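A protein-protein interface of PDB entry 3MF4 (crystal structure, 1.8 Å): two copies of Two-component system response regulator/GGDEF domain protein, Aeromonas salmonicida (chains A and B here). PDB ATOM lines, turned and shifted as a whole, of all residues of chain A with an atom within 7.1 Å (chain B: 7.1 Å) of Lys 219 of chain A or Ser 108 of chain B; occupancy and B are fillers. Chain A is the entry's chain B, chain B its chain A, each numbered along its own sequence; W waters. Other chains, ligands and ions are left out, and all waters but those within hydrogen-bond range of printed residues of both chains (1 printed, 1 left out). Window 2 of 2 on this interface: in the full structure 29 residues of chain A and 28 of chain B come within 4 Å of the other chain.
Printed residues of chain B within 4 Å of Arg 192 of chain A: His 107.
Of the printed residues of chain B, Leu 218 of chain A touches Tyr 111 (3.4 Å) and Glu 233 (3.4 Å).
Of the printed residues of chain B, Lys 219 of chain A touches Asp 99, Tyr 100, Ser 108 and Tyr 111.
Gly 221 of chain A touches none of the printed residues of chain B.
Of the printed residues of chain A, Ser 108 of chain B touches Lys 219.
Printed residues of chain A within 4 Å of Glu 233 of chain B: Ala 215 and Leu 218.
The nearest printed residue of chain A that does not touch Asp 99 of chain B is Ala 215 of chain A (7.7 Å).
No position is printed for both chains.
OD1 of Asp 99 of chain B lies within salt-bridge range of NZ of Lys 219 of chain A, 2.9 Å away.
The backbone carbonyl oxygen (O) of Tyr 100 of chain B sits at hydrogen-bond distance from the side-chain amino group (NZ) of Lys 219 of chain A (3.0 Å).
His 107 of chain B touches Arg 192 of chain A.
Ala 215 of chain A touches Glu 233 of chain B.
Tyr 111 of chain B touches Leu 218 of chain A (CD1 to O, 3.4 Å).
O of Glu 233 of chain B touches CD1 of Leu 218 of chain A, 3.4 Å away.
Ser 108 of chain B touches Lys 219 of chain A.
Lys 219 of chain A touches Tyr 111 of chain B.
Gln 220 of chain A touches His 107 of chain B (O to CD2, 3.2 Å).
Of the 20 printed residues of chain B, 6 touch a printed residue of chain A.
Printed residues of chain A that touch a printed residue of chain B: Arg 192, Ala 215, Leu 218, Lys 219 and Gln 220.
Among the printed residues, Asp or Glu carboxylates within 4 Å of a Lys or Arg side-chain nitrogen of the other chain: Lys 219 of chain A with Asp 99 of chain B (2.9 Å).
Water W1 lies within hydrogen-bond range of O of Ser 108 of chain B, N of Met 102 of chain B and O of Lys 219 of chain A.
The guanidinium group (NE) of Arg 89 of chain B lies within salt-bridge range of the side-chain carboxylate (OE2) of Glu 233 of chain B, 2.9 Å away.
OD2 of Asp 99 of chain B sits at hydrogen-bond distance from NE2 of Gln 236 of chain B, at 2.9 Å.
O of Met 102 of chain B lies within hydrogen-bond range of OG of Ser 108 of chain B, at 3.0 Å.
OD1 of Asp 104 of chain B lies within hydrogen-bond range of OG of Ser 108 of chain B.
OH of Tyr 111 of chain B is in hydrogen-bond range of NE2 of Gln 236 of chain B (2.8 Å).
The guanidinium group (NE) of Arg 192 of chain A lies within hydrogen-bond range of the backbone carbonyl oxygen (O) of Gly 221 of chain A, at 2.8 Å.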
ATOM      1  N   ARG A 192      20.082  15.438  11.118  1.00  0.00           N
ATOM      2  CA  ARG A 192      19.072  16.523  11.160  1.00  0.00           C
ATOM      3  C   ARG A 192      18.920  17.205  12.519  1.00  0.00           C
ATOM      4  O   ARG A 192      18.413  18.331  12.594  1.00  0.00           O
ATOM      5  CB  ARG A 192      17.747  15.989  10.687  1.00  0.00           C
ATOM      6  CG  ARG A 192      17.628  16.021   9.151  1.00  0.00           C
ATOM      7  CD  ARG A 192      17.491  17.442   8.589  1.00  0.00           C
ATOM      8  NE  ARG A 192      17.544  17.387   7.135  1.00  0.00           N
ATOM      9  CZ  ARG A 192      18.626  17.687   6.408  1.00  0.00           C
ATOM     10  NH1 ARG A 192      19.727  18.125   7.013  1.00  0.00           N
ATOM     11  NH2 ARG A 192      18.591  17.551   5.082  1.00  0.00           N
ATOM     12  N   LEU A 213       9.359   3.649   2.720  1.00  0.00           N
ATOM     13  CA  LEU A 213      10.645   4.182   3.140  1.00  0.00           C
ATOM     14  C   LEU A 213      10.879   5.613   2.651  1.00  0.00           C
ATOM     15  O   LEU A 213      11.300   6.466   3.417  1.00  0.00           O
ATOM     16  CB  LEU A 213      11.773   3.252   2.671  1.00  0.00           C
ATOM     17  CG  LEU A 213      11.871   1.884   3.365  1.00  0.00           C
ATOM     18  CD1 LEU A 213      12.881   0.975   2.668  1.00  0.00           C
ATOM     19  CD2 LEU A 213      12.231   2.033   4.838  1.00  0.00           C
ATOM     20  N   SER A 214      10.624   5.869   1.372  1.00  0.00           N
ATOM     21  CA  SER A 214      10.725   7.225   0.835  1.00  0.00           C
ATOM     22  C   SER A 214      10.011   8.244   1.717  1.00  0.00           C
ATOM     23  O   SER A 214      10.590   9.262   2.085  1.00  0.00           O
ATOM     24  CB  SER A 214      10.186   7.288  -0.594  1.00  0.00           C
ATOM     25  OG  SER A 214      11.201   6.926  -1.504  1.00  0.00           O
ATOM     26  N   ALA A 215       8.765   7.950   2.080  1.00  0.00           N
ATOM     27  CA  ALA A 215       8.004   8.812   2.981  1.00  0.00           C
ATOM     28  C   ALA A 215       8.714   9.000   4.326  1.00  0.00           C
ATOM     29  O   ALA A 215       8.823  10.121   4.823  1.00  0.00           O
ATOM     30  CB  ALA A 215       6.607   8.240   3.204  1.00  0.00           C
ATOM     31  N   ARG A 216       9.205   7.901   4.899  1.00  0.00           N
ATOM     32  CA  ARG A 216       9.909   7.954   6.176  1.00  0.00           C
ATOM     33  C   ARG A 216      11.122   8.894   6.112  1.00  0.00           C
ATOM     34  O   ARG A 216      11.298   9.733   7.004  1.00  0.00           O
ATOM     35  CB  ARG A 216      10.301   6.544   6.653  1.00  0.00           C
ATOM     36  CG  ARG A 216       9.165   5.791   7.367  1.00  0.00           C
ATOM     37  CD  ARG A 216       9.614   4.411   7.878  1.00  0.00           C
ATOM     38  NE  ARG A 216      10.492   4.487   9.046  1.00  0.00           N
ATOM     39  CZ  ARG A 216      11.295   3.498   9.442  1.00  0.00           C
ATOM     40  NH1 ARG A 216      11.338   2.358   8.755  1.00  0.00           N
ATOM     41  NH2 ARG A 216      12.060   3.650  10.518  1.00  0.00           N
ATOM     42  N   TYR A 217      11.926   8.780   5.052  1.00  0.00           N
ATOM     43  CA  TYR A 217      13.027   9.716   4.829  1.00  0.00           C
ATOM     44  C   TYR A 217      12.564  11.157   4.844  1.00  0.00           C
ATOM     45  O   TYR A 217      13.123  11.980   5.581  1.00  0.00           O
ATOM     46  CB  TYR A 217      13.732   9.452   3.508  1.00  0.00           C
ATOM     47  CG  TYR A 217      14.812   8.417   3.583  1.00  0.00           C
ATOM     48  CD1 TYR A 217      15.823   8.506   4.532  1.00  0.00           C
ATOM     49  CD2 TYR A 217      14.847   7.364   2.679  1.00  0.00           C
ATOM     50  CE1 TYR A 217      16.853   7.542   4.591  1.00  0.00           C
ATOM     51  CE2 TYR A 217      15.854   6.399   2.736  1.00  0.00           C
ATOM     52  CZ  TYR A 217      16.848   6.500   3.693  1.00  0.00           C
ATOM     53  OH  TYR A 217      17.858   5.560   3.735  1.00  0.00           O
ATOM     54  N   LEU A 218      11.561  11.450   4.016  1.00  0.00           N
ATOM     55  CA  LEU A 218      11.077  12.822   3.842  1.00  0.00           C
ATOM     56  C   LEU A 218      10.559  13.424   5.136  1.00  0.00           C
ATOM     57  O   LEU A 218      10.912  14.551   5.476  1.00  0.00           O
ATOM     58  CB  LEU A 218      10.029  12.909   2.738  1.00  0.00           C
ATOM     59  CG  LEU A 218      10.562  12.568   1.338  1.00  0.00           C
ATOM     60  CD1 LEU A 218       9.401  12.321   0.384  1.00  0.00           C
ATOM     61  CD2 LEU A 218      11.531  13.642   0.811  1.00  0.00           C
ATOM     62  N   LYS A 219       9.750  12.666   5.876  1.00  0.00           N
ATOM     63  CA  LYS A 219       9.230  13.148   7.158  1.00  0.00           C
ATOM     64  C   LYS A 219      10.290  13.341   8.244  1.00  0.00           C
ATOM     65  O   LYS A 219      10.059  14.095   9.200  1.00  0.00           O
ATOM     66  CB  LYS A 219       8.100  12.233   7.667  1.00  0.00           C
ATOM     67  CG  LYS A 219       6.878  12.211   6.762  1.00  0.00           C
ATOM     68  CD  LYS A 219       6.080  13.516   6.863  1.00  0.00           C
ATOM     69  CE  LYS A 219       5.131  13.719   5.668  1.00  0.00           C
ATOM     70  NZ  LYS A 219       4.042  12.707   5.623  1.00  0.00           N
ATOM     71  N   GLN A 220      11.432  12.659   8.095  1.00  0.00           N
ATOM     72  CA  GLN A 220      12.605  12.830   8.971  1.00  0.00           C
ATOM     73  C   GLN A 220      13.554  13.937   8.484  1.00  0.00           C
ATOM     74  O   GLN A 220      14.572  14.219   9.124  1.00  0.00           O
ATOM     75  CB  GLN A 220      13.402  11.527   9.106  1.00  0.00           C
ATOM     76  CG  GLN A 220      12.712  10.401   9.873  1.00  0.00           C
ATOM     77  CD  GLN A 220      12.614  10.638  11.378  1.00  0.00           C
ATOM     78  OE1 GLN A 220      13.332  11.475  11.948  1.00  0.00           O
ATOM     79  NE2 GLN A 220      11.725   9.895  12.032  1.00  0.00           N
ATOM     80  N   GLY A 221      13.216  14.561   7.357  1.00  0.00           N
ATOM     81  CA  GLY A 221      13.929  15.741   6.905  1.00  0.00           C
ATOM     82  C   GLY A 221      14.884  15.539   5.755  1.00  0.00           C
ATOM     83  O   GLY A 221      15.597  16.484   5.371  1.00  0.00           O
ATOM     84  N   ALA A 222      14.910  14.331   5.185  1.00  0.00           N
ATOM     85  CA  ALA A 222      15.638  14.134   3.927  1.00  0.00           C
ATOM     86  C   ALA A 222      15.120  15.164   2.916  1.00  0.00           C
ATOM     87  O   ALA A 222      13.915  15.451   2.880  1.00  0.00           O
ATOM     88  CB  ALA A 222      15.448  12.738   3.408  1.00  0.00           C
ATOM     89  N   THR B  81       1.439  14.565  14.568  1.00  0.00           N
ATOM     90  CA  THR B  81       1.470  13.264  15.231  1.00  0.00           C
ATOM     91  C   THR B  81       2.834  12.883  15.824  1.00  0.00           C
ATOM     92  O   THR B  81       3.854  13.131  15.224  1.00  0.00           O
ATOM     93  CB  THR B  81       0.897  12.128  14.304  1.00  0.00           C
ATOM     94  OG1 THR B  81       0.910  10.876  14.995  1.00  0.00           O
ATOM     95  CG2 THR B  81       1.650  12.003  12.993  1.00  0.00           C
ATOM     96  N   ARG B  89      -1.651   5.796   8.873  1.00  0.00           N
ATOM     97  CA  ARG B  89      -1.508   6.528   7.620  1.00  0.00           C
ATOM     98  C   ARG B  89      -2.715   6.303   6.707  1.00  0.00           C
ATOM     99  O   ARG B  89      -3.278   7.261   6.170  1.00  0.00           O
ATOM    100  CB  ARG B  89      -0.212   6.153   6.901  1.00  0.00           C
ATOM    101  CG  ARG B  89       0.196   7.174   5.856  1.00  0.00           C
ATOM    102  CD  ARG B  89       1.457   6.766   5.135  1.00  0.00           C
ATOM    103  NE  ARG B  89       1.439   7.238   3.755  1.00  0.00           N
ATOM    104  CZ  ARG B  89       0.961   6.537   2.730  1.00  0.00           C
ATOM    105  NH1 ARG B  89       0.465   5.315   2.916  1.00  0.00           N
ATOM    106  NH2 ARG B  89       0.988   7.056   1.511  1.00  0.00           N
ATOM    107  N   ASP B  99      -2.223  15.419   4.708  1.00  0.00           N
ATOM    108  CA  ASP B  99      -0.886  14.924   5.004  1.00  0.00           C
ATOM    109  C   ASP B  99      -0.743  14.871   6.522  1.00  0.00           C
ATOM    110  O   ASP B  99      -1.635  15.297   7.267  1.00  0.00           O
ATOM    111  CB  ASP B  99       0.180  15.863   4.369  1.00  0.00           C
ATOM    112  CG  ASP B  99       1.524  15.169   4.091  1.00  0.00           C
ATOM    113  OD1 ASP B  99       1.741  14.004   4.490  1.00  0.00           O
ATOM    114  OD2 ASP B  99       2.391  15.815   3.461  1.00  0.00           O
ATOM    115  N   TYR B 100       0.363  14.298   6.979  1.00  0.00           N
ATOM    116  CA  TYR B 100       0.702  14.315   8.382  1.00  0.00           C
ATOM    117  C   TYR B 100       2.144  14.791   8.537  1.00  0.00           C
ATOM    118  O   TYR B 100       2.946  14.691   7.598  1.00  0.00           O
ATOM    119  CB  TYR B 100       0.495  12.952   9.036  1.00  0.00           C
ATOM    120  CG  TYR B 100       1.459  11.882   8.570  1.00  0.00           C
ATOM    121  CD1 TYR B 100       2.591  11.579   9.318  1.00  0.00           C
ATOM    122  CD2 TYR B 100       1.237  11.165   7.388  1.00  0.00           C
ATOM    123  CE1 TYR B 100       3.487  10.589   8.909  1.00  0.00           C
ATOM    124  CE2 TYR B 100       2.133  10.175   6.973  1.00  0.00           C
ATOM    125  CZ  TYR B 100       3.250   9.893   7.738  1.00  0.00           C
ATOM    126  OH  TYR B 100       4.152   8.905   7.356  1.00  0.00           O
ATOM    127  N   VAL B 101       2.439  15.327   9.718  1.00  0.00           N
ATOM    128  CA  VAL B 101       3.750  15.863  10.066  1.00  0.00           C
ATOM    129  C   VAL B 101       4.142  15.225  11.391  1.00  0.00           C
ATOM    130  O   VAL B 101       3.346  15.196  12.326  1.00  0.00           O
ATOM    131  CB  VAL B 101       3.749  17.430  10.163  1.00  0.00           C
ATOM    132  CG1 VAL B 101       5.052  17.974  10.805  1.00  0.00           C
ATOM    133  CG2 VAL B 101       3.563  18.048   8.787  1.00  0.00           C
ATOM    134  N   MET B 102       5.339  14.642  11.437  1.00  0.00           N
ATOM    135  CA  MET B 102       5.887  14.082  12.661  1.00  0.00           C
ATOM    136  C   MET B 102       6.290  15.229  13.593  1.00  0.00           C
ATOM    137  O   MET B 102       6.961  16.163  13.178  1.00  0.00           O
ATOM    138  CB  MET B 102       7.105  13.192  12.365  1.00  0.00           C
ATOM    139  CG  MET B 102       6.820  12.002  11.450  1.00  0.00           C
ATOM    140  SD  MET B 102       5.379  10.838  12.081  1.00  0.00           S
ATOM    141  CE  MET B 102       5.914  10.466  13.878  1.00  0.00           C
ATOM    142  N   LYS B 103       5.863  15.171  14.843  1.00  0.00           N
ATOM    143  CA  LYS B 103       6.228  16.235  15.792  1.00  0.00           C
ATOM    144  C   LYS B 103       7.039  15.673  16.955  1.00  0.00           C
ATOM    145  O   LYS B 103       7.022  16.225  18.063  1.00  0.00           O
ATOM    146  CB  LYS B 103       4.978  16.996  16.276  1.00  0.00           C
ATOM    147  CG  LYS B 103       3.950  16.125  16.983  1.00  0.00           C
ATOM    148  CD  LYS B 103       3.180  16.891  18.024  1.00  0.00           C
ATOM    149  CE  LYS B 103       1.957  16.096  18.420  1.00  0.00           C
ATOM    150  NZ  LYS B 103       1.187  16.830  19.457  1.00  0.00           N
ATOM    151  N   ASP B 104       7.757  14.580  16.682  1.00  0.00           N
ATOM    152  CA  ASP B 104       8.632  13.919  17.672  1.00  0.00           C
ATOM    153  C   ASP B 104       9.978  14.637  17.881  1.00  0.00           C
ATOM    154  O   ASP B 104      10.674  14.408  18.868  1.00  0.00           O
ATOM    155  CB  ASP B 104       8.853  12.432  17.318  1.00  0.00           C
ATOM    156  CG  ASP B 104       9.566  12.231  15.993  1.00  0.00           C
ATOM    157  OD1 ASP B 104       9.180  12.874  15.001  1.00  0.00           O
ATOM    158  OD2 ASP B 104      10.525  11.416  15.937  1.00  0.00           O
ATOM    159  N   SER B 105      10.337  15.501  16.941  1.00  0.00           N
ATOM    160  CA  SER B 105      11.560  16.283  17.020  1.00  0.00           C
ATOM    161  C   SER B 105      11.347  17.606  16.317  1.00  0.00           C
ATOM    162  O   SER B 105      10.462  17.728  15.470  1.00  0.00           O
ATOM    163  CB  SER B 105      12.678  15.561  16.290  1.00  0.00           C
ATOM    164  OG  SER B 105      12.320  15.446  14.925  1.00  0.00           O
ATOM    165  N   ARG B 106      12.195  18.582  16.628  1.00  0.00           N
ATOM    166  CA  ARG B 106      12.099  19.879  15.981  1.00  0.00           C
ATOM    167  C   ARG B 106      12.356  19.782  14.466  1.00  0.00           C
ATOM    168  O   ARG B 106      11.668  20.430  13.691  1.00  0.00           O
ATOM    169  CB  ARG B 106      13.021  20.894  16.668  1.00  0.00           C
ATOM    170  CG  ARG B 106      13.146  22.229  15.965  1.00  0.00           C
ATOM    171  CD  ARG B 106      11.884  23.099  16.108  1.00  0.00           C
ATOM    172  NE  ARG B 106      12.026  24.316  15.315  1.00  0.00           N
ATOM    173  CZ  ARG B 106      11.823  24.391  14.000  1.00  0.00           C
ATOM    174  NH1 ARG B 106      11.435  23.317  13.312  1.00  0.00           N
ATOM    175  NH2 ARG B 106      11.999  25.546  13.367  1.00  0.00           N
ATOM    176  N   HIS B 107      13.328  18.967  14.038  1.00  0.00           N
ATOM    177  CA  HIS B 107      13.583  18.826  12.595  1.00  0.00           C
ATOM    178  C   HIS B 107      12.428  18.170  11.816  1.00  0.00           C
ATOM    179  O   HIS B 107      12.213  18.474  10.652  1.00  0.00           O
ATOM    180  CB  HIS B 107      14.915  18.116  12.295  1.00  0.00           C
ATOM    181  CG  HIS B 107      14.959  16.678  12.714  1.00  0.00           C
ATOM    182  ND1 HIS B 107      15.476  16.275  13.925  1.00  0.00           N
ATOM    183  CD2 HIS B 107      14.590  15.544  12.066  1.00  0.00           C
ATOM    184  CE1 HIS B 107      15.407  14.957  14.017  1.00  0.00           C
ATOM    185  NE2 HIS B 107      14.871  14.490  12.904  1.00  0.00           N
ATOM    186  N   SER B 108      11.685  17.262  12.440  1.00  0.00           N
ATOM    187  CA  SER B 108      10.556  16.641  11.752  1.00  0.00           C
ATOM    188  C   SER B 108       9.426  17.664  11.691  1.00  0.00           C
ATOM    189  O   SER B 108       8.710  17.751  10.704  1.00  0.00           O
ATOM    190  CB  SER B 108      10.107  15.363  12.460  1.00  0.00           C
ATOM    191  OG  SER B 108       9.824  15.598  13.831  1.00  0.00           O
ATOM    192  N   LEU B 109       9.319  18.451  12.755  1.00  0.00           N
ATOM    193  CA  LEU B 109       8.276  19.466  12.872  1.00  0.00           C
ATOM    194  C   LEU B 109       8.477  20.514  11.786  1.00  0.00           C
ATOM    195  O   LEU B 109       7.520  21.125  11.331  1.00  0.00           O
ATOM    196  CB  LEU B 109       8.365  20.137  14.242  1.00  0.00           C
ATOM    197  CG  LEU B 109       7.149  20.480  15.104  1.00  0.00           C
ATOM    198  CD1 LEU B 109       7.458  21.805  15.783  1.00  0.00           C
ATOM    199  CD2 LEU B 109       5.773  20.527  14.381  1.00  0.00           C
ATOM    200  N   GLN B 110       9.726  20.703  11.364  1.00  0.00           N
ATOM    201  CA  GLN B 110      10.058  21.685  10.318  1.00  0.00           C
ATOM    202  C   GLN B 110       9.367  21.372   8.975  1.00  0.00           C
ATOM    203  O   GLN B 110       9.114  22.278   8.161  1.00  0.00           O
ATOM    204  CB  GLN B 110      11.587  21.761  10.147  1.00  0.00           C
ATOM    205  CG  GLN B 110      12.093  22.859   9.208  1.00  0.00           C
ATOM    206  CD  GLN B 110      11.688  24.285   9.624  1.00  0.00           C
ATOM    207  OE1 GLN B 110      11.581  24.613  10.814  1.00  0.00           O
ATOM    208  NE2 GLN B 110      11.478  25.139   8.627  1.00  0.00           N
ATOM    209  N   TYR B 111       9.041  20.097   8.761  1.00  0.00           N
ATOM    210  CA  TYR B 111       8.313  19.654   7.558  1.00  0.00           C
ATOM    211  C   TYR B 111       7.011  20.462   7.389  1.00  0.00           C
ATOM    212  O   TYR B 111       6.673  20.884   6.284  1.00  0.00           O
ATOM    213  CB  TYR B 111       8.014  18.148   7.645  1.00  0.00           C
ATOM    214  CG  TYR B 111       7.469  17.536   6.366  1.00  0.00           C
ATOM    215  CD1 TYR B 111       8.291  16.780   5.533  1.00  0.00           C
ATOM    216  CD2 TYR B 111       6.134  17.710   5.991  1.00  0.00           C
ATOM    217  CE1 TYR B 111       7.805  16.211   4.351  1.00  0.00           C
ATOM    218  CE2 TYR B 111       5.635  17.149   4.801  1.00  0.00           C
ATOM    219  CZ  TYR B 111       6.484  16.400   3.996  1.00  0.00           C
ATOM    220  OH  TYR B 111       6.027  15.834   2.831  1.00  0.00           O
ATOM    221  N   ALA B 112       6.317  20.702   8.501  1.00  0.00           N
ATOM    222  CA  ALA B 112       5.105  21.518   8.515  1.00  0.00           C
ATOM    223  C   ALA B 112       5.307  22.918   7.947  1.00  0.00           C
ATOM    224  O   ALA B 112       4.397  23.461   7.321  1.00  0.00           O
ATOM    225  CB  ALA B 112       4.522  21.596   9.941  1.00  0.00           C
ATOM    226  N   VAL B 113       6.489  23.497   8.178  1.00  0.00           N
ATOM    227  CA  VAL B 113       6.765  24.878   7.779  1.00  0.00           C
ATOM    228  C   VAL B 113       6.898  25.011   6.269  1.00  0.00           C
ATOM    229  O   VAL B 113       6.279  25.886   5.661  1.00  0.00           O
ATOM    230  CB  VAL B 113       8.000  25.462   8.492  1.00  0.00           C
ATOM    231  CG1 VAL B 113       8.212  26.938   8.097  1.00  0.00           C
ATOM    232  CG2 VAL B 113       7.819  25.336   9.988  1.00  0.00           C
ATOM    233  N   LEU B 115       5.711  22.848   4.235  1.00  0.00           N
ATOM    234  CA  LEU B 115       4.430  22.395   3.674  1.00  0.00           C
ATOM    235  C   LEU B 115       3.411  23.534   3.622  1.00  0.00           C
ATOM    236  O   LEU B 115       2.790  23.715   2.608  1.00  0.00           O
ATOM    237  CB  LEU B 115       3.879  21.169   4.425  1.00  0.00           C
ATOM    238  CG  LEU B 115       2.560  20.467   4.077  1.00  0.00           C
ATOM    239  CD1 LEU B 115       2.490  19.881   2.653  1.00  0.00           C
ATOM    240  CD2 LEU B 115       2.296  19.358   5.118  1.00  0.00           C
ATOM    241  N   GLU B 233       3.746  11.006  -1.016  1.00  0.00           N
ATOM    242  CA  GLU B 233       4.849  11.788  -0.443  1.00  0.00           C
ATOM    243  C   GLU B 233       5.961  12.028  -1.473  1.00  0.00           C
ATOM    244  O   GLU B 233       6.627  13.062  -1.435  1.00  0.00           O
ATOM    245  CB  GLU B 233       5.430  11.103   0.799  1.00  0.00           C
ATOM    246  CG  GLU B 233       4.486  11.032   2.005  1.00  0.00           C
ATOM    247  CD  GLU B 233       3.684   9.727   2.093  1.00  0.00           C
ATOM    248  OE1 GLU B 233       3.417   9.078   1.052  1.00  0.00           O
ATOM    249  OE2 GLU B 233       3.298   9.358   3.226  1.00  0.00           O
ATOM    250  N   GLN B 236       4.530  14.746  -3.985  1.00  0.00           N
ATOM    251  CA  GLN B 236       4.564  16.081  -3.348  1.00  0.00           C
ATOM    252  C   GLN B 236       5.973  16.658  -3.300  1.00  0.00           C
ATOM    253  O   GLN B 236       6.185  17.840  -3.569  1.00  0.00           O
ATOM    254  CB  GLN B 236       3.946  15.986  -1.953  1.00  0.00           C
ATOM    255  CG  GLN B 236       3.793  17.268  -1.176  1.00  0.00           C
ATOM    256  CD  GLN B 236       3.149  17.017   0.179  1.00  0.00           C
ATOM    257  OE1 GLN B 236       1.937  17.206   0.350  1.00  0.00           O
ATOM    258  NE2 GLN B 236       3.945  16.550   1.139  1.00  0.00           N
HETATM  259  O   HOH W   1       7.540  15.373   9.741  1.00  0.00           O
